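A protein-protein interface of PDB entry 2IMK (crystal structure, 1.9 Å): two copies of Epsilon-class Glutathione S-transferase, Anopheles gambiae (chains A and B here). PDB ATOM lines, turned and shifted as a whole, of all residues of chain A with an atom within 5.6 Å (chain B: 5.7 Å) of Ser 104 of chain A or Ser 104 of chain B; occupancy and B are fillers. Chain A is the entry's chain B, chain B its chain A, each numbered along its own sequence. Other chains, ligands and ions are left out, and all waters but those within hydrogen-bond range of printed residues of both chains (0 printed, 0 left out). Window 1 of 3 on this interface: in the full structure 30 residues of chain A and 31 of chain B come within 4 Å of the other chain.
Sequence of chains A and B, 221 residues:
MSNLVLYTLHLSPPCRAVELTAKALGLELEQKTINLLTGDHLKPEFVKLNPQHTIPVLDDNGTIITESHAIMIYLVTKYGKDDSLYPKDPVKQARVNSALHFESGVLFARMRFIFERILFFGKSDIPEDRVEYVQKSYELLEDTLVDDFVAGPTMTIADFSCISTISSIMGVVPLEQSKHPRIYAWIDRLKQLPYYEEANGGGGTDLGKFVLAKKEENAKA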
ATOM      1  N   GLU A  67      21.194   9.270   8.097  1.00  0.00           N
ATOM      2  CA  GLU A  67      21.062  10.644   7.530  1.00  0.00           C
ATOM      3  C   GLU A  67      22.388  11.238   7.026  1.00  0.00           C
ATOM      4  O   GLU A  67      23.325  11.439   7.814  1.00  0.00           O
ATOM      5  CB  GLU A  67      20.384  11.575   8.551  1.00  0.00           C
ATOM      6  CG  GLU A  67      19.518  12.630   7.910  1.00  0.00           C
ATOM      7  CD  GLU A  67      20.320  13.821   7.473  1.00  0.00           C
ATOM      8  OE1 GLU A  67      19.931  14.470   6.471  1.00  0.00           O
ATOM      9  OE2 GLU A  67      21.375  14.068   8.105  1.00  0.00           O
ATOM     10  N   HIS A  69      23.648  14.149   6.242  1.00  0.00           N
ATOM     11  CA  HIS A  69      24.370  15.306   6.780  1.00  0.00           C
ATOM     12  C   HIS A  69      24.967  14.955   8.129  1.00  0.00           C
ATOM     13  O   HIS A  69      26.113  15.354   8.425  1.00  0.00           O
ATOM     14  CB  HIS A  69      23.443  16.560   6.889  1.00  0.00           C
ATOM     15  CG  HIS A  69      22.689  16.869   5.621  1.00  0.00           C
ATOM     16  ND1 HIS A  69      21.478  16.297   5.324  1.00  0.00           N
ATOM     17  CD2 HIS A  69      23.012  17.642   4.558  1.00  0.00           C
ATOM     18  CE1 HIS A  69      21.078  16.709   4.132  1.00  0.00           C
ATOM     19  NE2 HIS A  69      21.984  17.543   3.660  1.00  0.00           N
ATOM     20  N   ALA A  99      23.730  26.196   5.474  1.00  0.00           N
ATOM     21  CA  ALA A  99      23.746  25.667   4.097  1.00  0.00           C
ATOM     22  C   ALA A  99      23.286  24.158   4.024  1.00  0.00           C
ATOM     23  O   ALA A  99      22.566  23.766   3.078  1.00  0.00           O
ATOM     24  CB  ALA A  99      25.142  25.844   3.460  1.00  0.00           C
ATOM     25  N   LEU A 100      23.695  23.337   4.994  1.00  0.00           N
ATOM     26  CA  LEU A 100      23.147  21.944   5.099  1.00  0.00           C
ATOM     27  C   LEU A 100      21.621  21.814   5.247  1.00  0.00           C
ATOM     28  O   LEU A 100      21.007  20.990   4.591  1.00  0.00           O
ATOM     29  CB  LEU A 100      23.841  21.179   6.241  1.00  0.00           C
ATOM     30  CG  LEU A 100      25.355  20.962   6.123  1.00  0.00           C
ATOM     31  CD1 LEU A 100      25.894  20.407   7.502  1.00  0.00           C
ATOM     32  CD2 LEU A 100      25.820  20.080   4.922  1.00  0.00           C
ATOM     33  N   HIS A 101      21.016  22.617   6.131  1.00  0.00           N
ATOM     34  CA  HIS A 101      19.584  22.714   6.204  1.00  0.00           C
ATOM     35  C   HIS A 101      18.879  23.319   4.959  1.00  0.00           C
ATOM     36  O   HIS A 101      17.747  22.950   4.617  1.00  0.00           O
ATOM     37  CB  HIS A 101      19.195  23.407   7.538  1.00  0.00           C
ATOM     38  CG  HIS A 101      19.458  22.540   8.711  1.00  0.00           C
ATOM     39  ND1 HIS A 101      18.632  21.491   9.031  1.00  0.00           N
ATOM     40  CD2 HIS A 101      20.520  22.453   9.548  1.00  0.00           C
ATOM     41  CE1 HIS A 101      19.143  20.829  10.059  1.00  0.00           C
ATOM     42  NE2 HIS A 101      20.291  21.394  10.389  1.00  0.00           N
ATOM     43  N   PHE A 102      19.569  24.218   4.263  1.00  0.00           N
ATOM     44  CA  PHE A 102      19.064  24.726   2.994  1.00  0.00           C
ATOM     45  C   PHE A 102      18.990  23.525   2.064  1.00  0.00           C
ATOM     46  O   PHE A 102      17.997  23.354   1.355  1.00  0.00           O
ATOM     47  CB  PHE A 102      19.928  25.859   2.411  1.00  0.00           C
ATOM     48  CG  PHE A 102      19.495  26.302   1.024  1.00  0.00           C
ATOM     49  CD1 PHE A 102      18.254  26.992   0.834  1.00  0.00           C
ATOM     50  CD2 PHE A 102      20.291  26.004  -0.069  1.00  0.00           C
ATOM     51  CE1 PHE A 102      17.816  27.389  -0.420  1.00  0.00           C
ATOM     52  CE2 PHE A 102      19.871  26.398  -1.370  1.00  0.00           C
ATOM     53  CZ  PHE A 102      18.647  27.063  -1.541  1.00  0.00           C
ATOM     54  N   GLU A 103      20.030  22.701   2.048  1.00  0.00           N
ATOM     55  CA  GLU A 103      20.041  21.583   1.141  1.00  0.00           C
ATOM     56  C   GLU A 103      18.937  20.591   1.497  1.00  0.00           C
ATOM     57  O   GLU A 103      18.236  20.100   0.624  1.00  0.00           O
ATOM     58  CB  GLU A 103      21.432  20.922   1.048  1.00  0.00           C
ATOM     59  CG  GLU A 103      21.614  20.068  -0.225  1.00  0.00           C
ATOM     60  CD  GLU A 103      20.940  18.670  -0.176  1.00  0.00           C
ATOM     61  OE1 GLU A 103      20.833  17.990  -1.246  1.00  0.00           O
ATOM     62  OE2 GLU A 103      20.571  18.219   0.930  1.00  0.00           O
ATOM     63  N   SER A 104      18.739  20.297   2.778  1.00  0.00           N
ATOM     64  CA  SER A 104      17.743  19.275   3.141  1.00  0.00           C
ATOM     65  C   SER A 104      16.281  19.826   3.073  1.00  0.00           C
ATOM     66  O   SER A 104      15.364  19.182   2.450  1.00  0.00           O
ATOM     67  CB  SER A 104      18.149  18.619   4.467  1.00  0.00           C
ATOM     68  OG  SER A 104      17.837  19.426   5.589  1.00  0.00           O
ATOM     69  N   GLY A 105      16.041  21.009   3.661  1.00  0.00           N
ATOM     70  CA  GLY A 105      14.691  21.622   3.644  1.00  0.00           C
ATOM     71  C   GLY A 105      14.240  22.282   2.337  1.00  0.00           C
ATOM     72  O   GLY A 105      13.048  22.461   2.125  1.00  0.00           O
ATOM     73  N   VAL A 106      15.170  22.614   1.434  1.00  0.00           N
ATOM     74  CA  VAL A 106      14.816  23.332   0.201  1.00  0.00           C
ATOM     75  C   VAL A 106      15.244  22.529  -1.051  1.00  0.00           C
ATOM     76  O   VAL A 106      14.379  22.109  -1.849  1.00  0.00           O
ATOM     77  CB  VAL A 106      15.312  24.797   0.178  1.00  0.00           C
ATOM     78  CG1 VAL A 106      15.050  25.448  -1.157  1.00  0.00           C
ATOM     79  CG2 VAL A 106      14.694  25.602   1.375  1.00  0.00           C
ATOM     80  N   LEU A 107      16.534  22.270  -1.203  1.00  0.00           N
ATOM     81  CA  LEU A 107      17.002  21.722  -2.487  1.00  0.00           C
ATOM     82  C   LEU A 107      16.537  20.268  -2.645  1.00  0.00           C
ATOM     83  O   LEU A 107      15.877  19.928  -3.655  1.00  0.00           O
ATOM     84  CB  LEU A 107      18.511  21.818  -2.596  1.00  0.00           C
ATOM     85  CG  LEU A 107      19.183  23.187  -2.912  1.00  0.00           C
ATOM     86  CD1 LEU A 107      20.707  22.990  -3.083  1.00  0.00           C
ATOM     87  CD2 LEU A 107      18.587  23.794  -4.204  1.00  0.00           C
ATOM     88  N   PHE A 108      16.905  19.421  -1.681  1.00  0.00           N
ATOM     89  CA  PHE A 108      16.520  18.011  -1.728  1.00  0.00           C
ATOM     90  C   PHE A 108      14.995  17.771  -1.601  1.00  0.00           C
ATOM     91  O   PHE A 108      14.459  17.013  -2.391  1.00  0.00           O
ATOM     92  CB  PHE A 108      17.296  17.207  -0.709  1.00  0.00           C
ATOM     93  CG  PHE A 108      16.945  15.774  -0.703  1.00  0.00           C
ATOM     94  CD1 PHE A 108      16.095  15.268   0.244  1.00  0.00           C
ATOM     95  CD2 PHE A 108      17.490  14.895  -1.668  1.00  0.00           C
ATOM     96  CE1 PHE A 108      15.760  13.896   0.254  1.00  0.00           C
ATOM     97  CE2 PHE A 108      17.150  13.562  -1.698  1.00  0.00           C
ATOM     98  CZ  PHE A 108      16.302  13.032  -0.742  1.00  0.00           C
ATOM     99  N   ALA A 109      14.324  18.356  -0.584  1.00  0.00           N
ATOM    100  CA  ALA A 109      12.862  18.339  -0.443  1.00  0.00           C
ATOM    101  C   ALA A 109      12.085  18.640  -1.734  1.00  0.00           C
ATOM    102  O   ALA A 109      11.151  17.909  -2.105  1.00  0.00           O
ATOM    103  CB  ALA A 109      12.391  19.362   0.712  1.00  0.00           C
ATOM    104  N   GLU B  67      19.106  30.781   9.869  1.00  0.00           N
ATOM    105  CA  GLU B  67      18.578  29.403   9.727  1.00  0.00           C
ATOM    106  C   GLU B  67      18.389  28.824  11.121  1.00  0.00           C
ATOM    107  O   GLU B  67      19.363  28.770  11.854  1.00  0.00           O
ATOM    108  CB  GLU B  67      19.456  28.533   8.815  1.00  0.00           C
ATOM    109  CG  GLU B  67      18.705  27.321   8.189  1.00  0.00           C
ATOM    110  CD  GLU B  67      18.379  26.193   9.175  1.00  0.00           C
ATOM    111  OE1 GLU B  67      17.321  25.542   8.979  1.00  0.00           O
ATOM    112  OE2 GLU B  67      19.178  25.951  10.148  1.00  0.00           O
ATOM    113  N   HIS B  69      18.207  26.066  12.795  1.00  0.00           N
ATOM    114  CA  HIS B  69      18.942  24.909  13.351  1.00  0.00           C
ATOM    115  C   HIS B  69      20.365  25.352  13.621  1.00  0.00           C
ATOM    116  O   HIS B  69      20.876  25.123  14.706  1.00  0.00           O
ATOM    117  CB  HIS B  69      18.876  23.649  12.464  1.00  0.00           C
ATOM    118  CG  HIS B  69      17.482  23.301  12.048  1.00  0.00           C
ATOM    119  ND1 HIS B  69      16.701  22.382  12.727  1.00  0.00           N
ATOM    120  CD2 HIS B  69      16.716  23.773  11.037  1.00  0.00           C
ATOM    121  CE1 HIS B  69      15.514  22.302  12.147  1.00  0.00           C
ATOM    122  NE2 HIS B  69      15.495  23.140  11.125  1.00  0.00           N
ATOM    123  N   ALA B  99      18.012  13.994  13.716  1.00  0.00           N
ATOM    124  CA  ALA B  99      16.659  14.523  13.962  1.00  0.00           C
ATOM    125  C   ALA B  99      16.446  15.978  13.408  1.00  0.00           C
ATOM    126  O   ALA B  99      15.418  16.266  12.793  1.00  0.00           O
ATOM    127  CB  ALA B  99      16.310  14.432  15.505  1.00  0.00           C
ATOM    128  N   LEU B 100      17.410  16.872  13.563  1.00  0.00           N
ATOM    129  CA  LEU B 100      17.323  18.221  12.969  1.00  0.00           C
ATOM    130  C   LEU B 100      17.082  18.236  11.466  1.00  0.00           C
ATOM    131  O   LEU B 100      16.269  19.015  10.954  1.00  0.00           O
ATOM    132  CB  LEU B 100      18.616  19.046  13.336  1.00  0.00           C
ATOM    133  CG  LEU B 100      18.936  19.302  14.814  1.00  0.00           C
ATOM    134  CD1 LEU B 100      20.438  19.776  14.981  1.00  0.00           C
ATOM    135  CD2 LEU B 100      17.917  20.293  15.386  1.00  0.00           C
ATOM    136  N   HIS B 101      17.796  17.391  10.736  1.00  0.00           N
ATOM    137  CA  HIS B 101      17.591  17.231   9.248  1.00  0.00           C
ATOM    138  C   HIS B 101      16.355  16.483   8.895  1.00  0.00           C
ATOM    139  O   HIS B 101      15.760  16.722   7.894  1.00  0.00           O
ATOM    140  CB  HIS B 101      18.776  16.565   8.670  1.00  0.00           C
ATOM    141  CG  HIS B 101      19.904  17.523   8.510  1.00  0.00           C
ATOM    142  ND1 HIS B 101      19.876  18.527   7.559  1.00  0.00           N
ATOM    143  CD2 HIS B 101      21.039  17.699   9.228  1.00  0.00           C
ATOM    144  CE1 HIS B 101      20.964  19.278   7.698  1.00  0.00           C
ATOM    145  NE2 HIS B 101      21.678  18.795   8.707  1.00  0.00           N
ATOM    146  N   PHE B 102      15.879  15.650   9.827  1.00  0.00           N
ATOM    147  CA  PHE B 102      14.535  15.141   9.682  1.00  0.00           C
ATOM    148  C   PHE B 102      13.502  16.257   9.903  1.00  0.00           C
ATOM    149  O   PHE B 102      12.576  16.343   9.130  1.00  0.00           O
ATOM    150  CB  PHE B 102      14.308  13.955  10.625  1.00  0.00           C
ATOM    151  CG  PHE B 102      12.880  13.498  10.685  1.00  0.00           C
ATOM    152  CD1 PHE B 102      12.362  12.689   9.685  1.00  0.00           C
ATOM    153  CD2 PHE B 102      12.068  13.900  11.751  1.00  0.00           C
ATOM    154  CE1 PHE B 102      10.989  12.273   9.754  1.00  0.00           C
ATOM    155  CE2 PHE B 102      10.758  13.487  11.826  1.00  0.00           C
ATOM    156  CZ  PHE B 102      10.212  12.701  10.827  1.00  0.00           C
ATOM    157  N   GLU B 103      13.666  17.120  10.897  1.00  0.00           N
ATOM    158  CA  GLU B 103      12.749  18.271  10.964  1.00  0.00           C
ATOM    159  C   GLU B 103      12.762  19.222   9.732  1.00  0.00           C
ATOM    160  O   GLU B 103      11.720  19.485   9.143  1.00  0.00           O
ATOM    161  CB  GLU B 103      12.844  19.017  12.304  1.00  0.00           C
ATOM    162  CG  GLU B 103      11.557  19.838  12.549  1.00  0.00           C
ATOM    163  CD  GLU B 103      11.576  21.215  11.890  1.00  0.00           C
ATOM    164  OE1 GLU B 103      12.572  21.559  11.181  1.00  0.00           O
ATOM    165  OE2 GLU B 103      10.608  21.982  12.090  1.00  0.00           O
ATOM    166  N   SER B 104      13.927  19.700   9.299  1.00  0.00           N
ATOM    167  CA  SER B 104      13.982  20.564   8.117  1.00  0.00           C
ATOM    168  C   SER B 104      13.521  19.844   6.798  1.00  0.00           C
ATOM    169  O   SER B 104      12.716  20.413   6.041  1.00  0.00           O
ATOM    170  CB  SER B 104      15.374  21.245   8.004  1.00  0.00           C
ATOM    171  OG  SER B 104      16.382  20.310   7.630  1.00  0.00           O
ATOM    172  N   GLY B 105      13.964  18.590   6.563  1.00  0.00           N
ATOM    173  CA  GLY B 105      13.812  17.953   5.251  1.00  0.00           C
ATOM    174  C   GLY B 105      12.467  17.258   5.128  1.00  0.00           C
ATOM    175  O   GLY B 105      11.972  17.012   3.998  1.00  0.00           O
ATOM    176  N   VAL B 106      11.884  16.922   6.291  1.00  0.00           N
ATOM    177  CA  VAL B 106      10.600  16.173   6.325  1.00  0.00           C
ATOM    178  C   VAL B 106       9.462  16.954   6.987  1.00  0.00           C
ATOM    179  O   VAL B 106       8.538  17.309   6.292  1.00  0.00           O
ATOM    180  CB  VAL B 106      10.726  14.696   6.864  1.00  0.00           C
ATOM    181  CG1 VAL B 106       9.373  13.912   6.782  1.00  0.00           C
ATOM    182  CG2 VAL B 106      11.860  13.947   6.077  1.00  0.00           C
ATOM    183  N   LEU B 107       9.510  17.200   8.288  1.00  0.00           N
ATOM    184  CA  LEU B 107       8.391  17.837   8.989  1.00  0.00           C
ATOM    185  C   LEU B 107       8.082  19.290   8.506  1.00  0.00           C
ATOM    186  O   LEU B 107       6.949  19.616   8.107  1.00  0.00           O
ATOM    187  CB  LEU B 107       8.605  17.788  10.508  1.00  0.00           C
ATOM    188  CG  LEU B 107       8.775  16.401  11.188  1.00  0.00           C
ATOM    189  CD1 LEU B 107       9.028  16.623  12.671  1.00  0.00           C
ATOM    190  CD2 LEU B 107       7.520  15.553  10.970  1.00  0.00           C
ATOM    191  N   PHE B 108       9.069  20.166   8.556  1.00  0.00           N
ATOM    192  CA  PHE B 108       8.881  21.490   8.026  1.00  0.00           C
ATOM    193  C   PHE B 108       8.644  21.572   6.522  1.00  0.00           C
ATOM    194  O   PHE B 108       7.767  22.333   6.111  1.00  0.00           O
ATOM    195  CB  PHE B 108      10.016  22.447   8.458  1.00  0.00           C
ATOM    196  CG  PHE B 108       9.755  23.904   8.096  1.00  0.00           C
ATOM    197  CD1 PHE B 108      10.319  24.462   6.959  1.00  0.00           C
ATOM    198  CD2 PHE B 108       8.929  24.695   8.895  1.00  0.00           C
ATOM    199  CE1 PHE B 108      10.058  25.788   6.622  1.00  0.00           C
ATOM    200  CE2 PHE B 108       8.659  25.991   8.585  1.00  0.00           C
ATOM    201  CZ  PHE B 108       9.215  26.573   7.496  1.00  0.00           C
ATOM    202  N   ALA B 109       9.398  20.845   5.691  1.00  0.00           N
ATOM    203  CA  ALA B 109       9.248  21.053   4.232  1.00  0.00           C
ATOM    204  C   ALA B 109       7.822  20.634   3.763  1.00  0.00           C
ATOM    205  O   ALA B 109       7.195  21.306   2.950  1.00  0.00           O
ATOM    206  CB  ALA B 109      10.321  20.291   3.480  1.00  0.00           C
ATOM    207  N   SER B 161      12.686  22.094  17.642  1.00  0.00           N
ATOM    208  CA  SER B 161      12.467  22.166  16.227  1.00  0.00           C
ATOM    209  C   SER B 161      11.226  21.298  15.789  1.00  0.00           C
ATOM    210  O   SER B 161      10.287  21.771  15.030  1.00  0.00           O
ATOM    211  CB  SER B 161      13.781  21.719  15.656  1.00  0.00           C
ATOM    212  OG  SER B 161      13.798  21.762  14.281  1.00  0.00           O
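Of the 13 printed residues of chain A, 7 touch a printed residue of chain B.
Hydrophobic or aromatic side chains of chain A that line the printed part of chain B: His 69, Leu 100, His 101 and Ala 109.
Among the printed residues, no Asp or Glu carboxylate lies within 4 Å of a Lys or Arg side-chain nitrogen of the other chain.
OG of Ser 104 of chain B is in hydrogen-bond range of ND1 of His 101 of chain A, 2.9 Å away.
OG of Ser 104 of chain A is in hydrogen-bond range of ND1 of His 101 of chain B, at 3.0 Å.
NE2 of His 101 of chain B sits at hydrogen-bond distance from NE2 of His 101 of chain A.
OG of Ser 104 of chain B is in hydrogen-bond range of OG of Ser 104 of chain A.
Glu 67 of chain A touches His 101 of chain B, and with the chains exchanged His 101 of chain A touches Glu 67 of chain B.
Leu 100 of chain A touches His 101 of chain B, and with the chains exchanged His 101 of chain A touches Leu 100 of chain B.
Ser 104 of chain A touches its own counterpart, Ser 104 of chain B.
Ala 109 of chain B touches its own counterpart, Ala 109 of chain A.
13 positions are printed for both chains.
Glu 67 of chain A touches His 101 of chain B (OE1 to CB, 3.2 Å).
His 69 of chain A touches His 101 of chain B (CB to NE2, 3.4 Å).
Leu 100 of chain A touches His 101 of chain B (O to CE1, 3.5 Å).
His 101 of chain A touches Glu 67 of chain B (CB to OE1, 3.2 Å).
His 101 of chain A touches His 69 of chain B (NE2 to CB, 3.4 Å).
His 101 of chain A touches Leu 100 of chain B.
O of Ser 104 of chain A touches CA of Gly 105 of chain B, at 3.4 Å.
Gly 105 of chain A touches Ser 104 of chain B.
CB of Ala 109 of chain B touches O of Gly 105 of chain A, at 3.7 Å.
Ala 109 of chain A touches Ala 109 of chain B (CB to CB, 3.6 Å).
Of the printed residues of chain B, Glu 67 of chain A touches His 101 (3.2 Å).
Printed residues of chain B within 4 Å of His 69 of chain A: His 101 (3.4 Å).
Printed residues of chain B within 4 Å of Ser 104 of chain A: His 101, Ser 104 and Gly 105.
Ser 104 of chain B touches just these residues of chain A: His 101 (2.9 Å), Ser 104 (2.7 Å) and Gly 105 (3.3 Å).
Printed residues of chain A within 4 Å of Gly 105 of chain B: Ser 104.
The nearest residue of chain B that does not touch Ser 104 of chain A is Ala 109 of chain B (5.3 Å).
The nearest residue of chain A that does not touch Ser 104 of chain B is Ala 109 of chain A (5.4 Å).
OE1 of Glu 67 of chain A sits at hydrogen-bond distance from ND1 of His 69 of chain A, at 2.7 Å.
The side-chain carboxylate (OE2) of Glu 67 of chain B lies within hydrogen-bond range of the backbone NH (N) of His 69 of chain B, 2.8 Å away.
The backbone carbonyl oxygen (O) of Ser 104 of chain A is in hydrogen-bond range of the backbone NH (N) of Ala 109 of chain A (3.3 Å).
OE2 of Glu 103 of chain A lies within hydrogen-bond range of NE2 of His 69 of chain A, at 3.1 Å.
A ring nitrogen (NE2) of His 69 of chain B lies close to the side-chain carboxylate of Glu 103 of chain B, at 3.3 Å.
The backbone NH of Ala 109 of chain B sits at hydrogen-bond distance from the backbone carbonyl oxygen of Ser 104 of chain B (3.4 Å).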
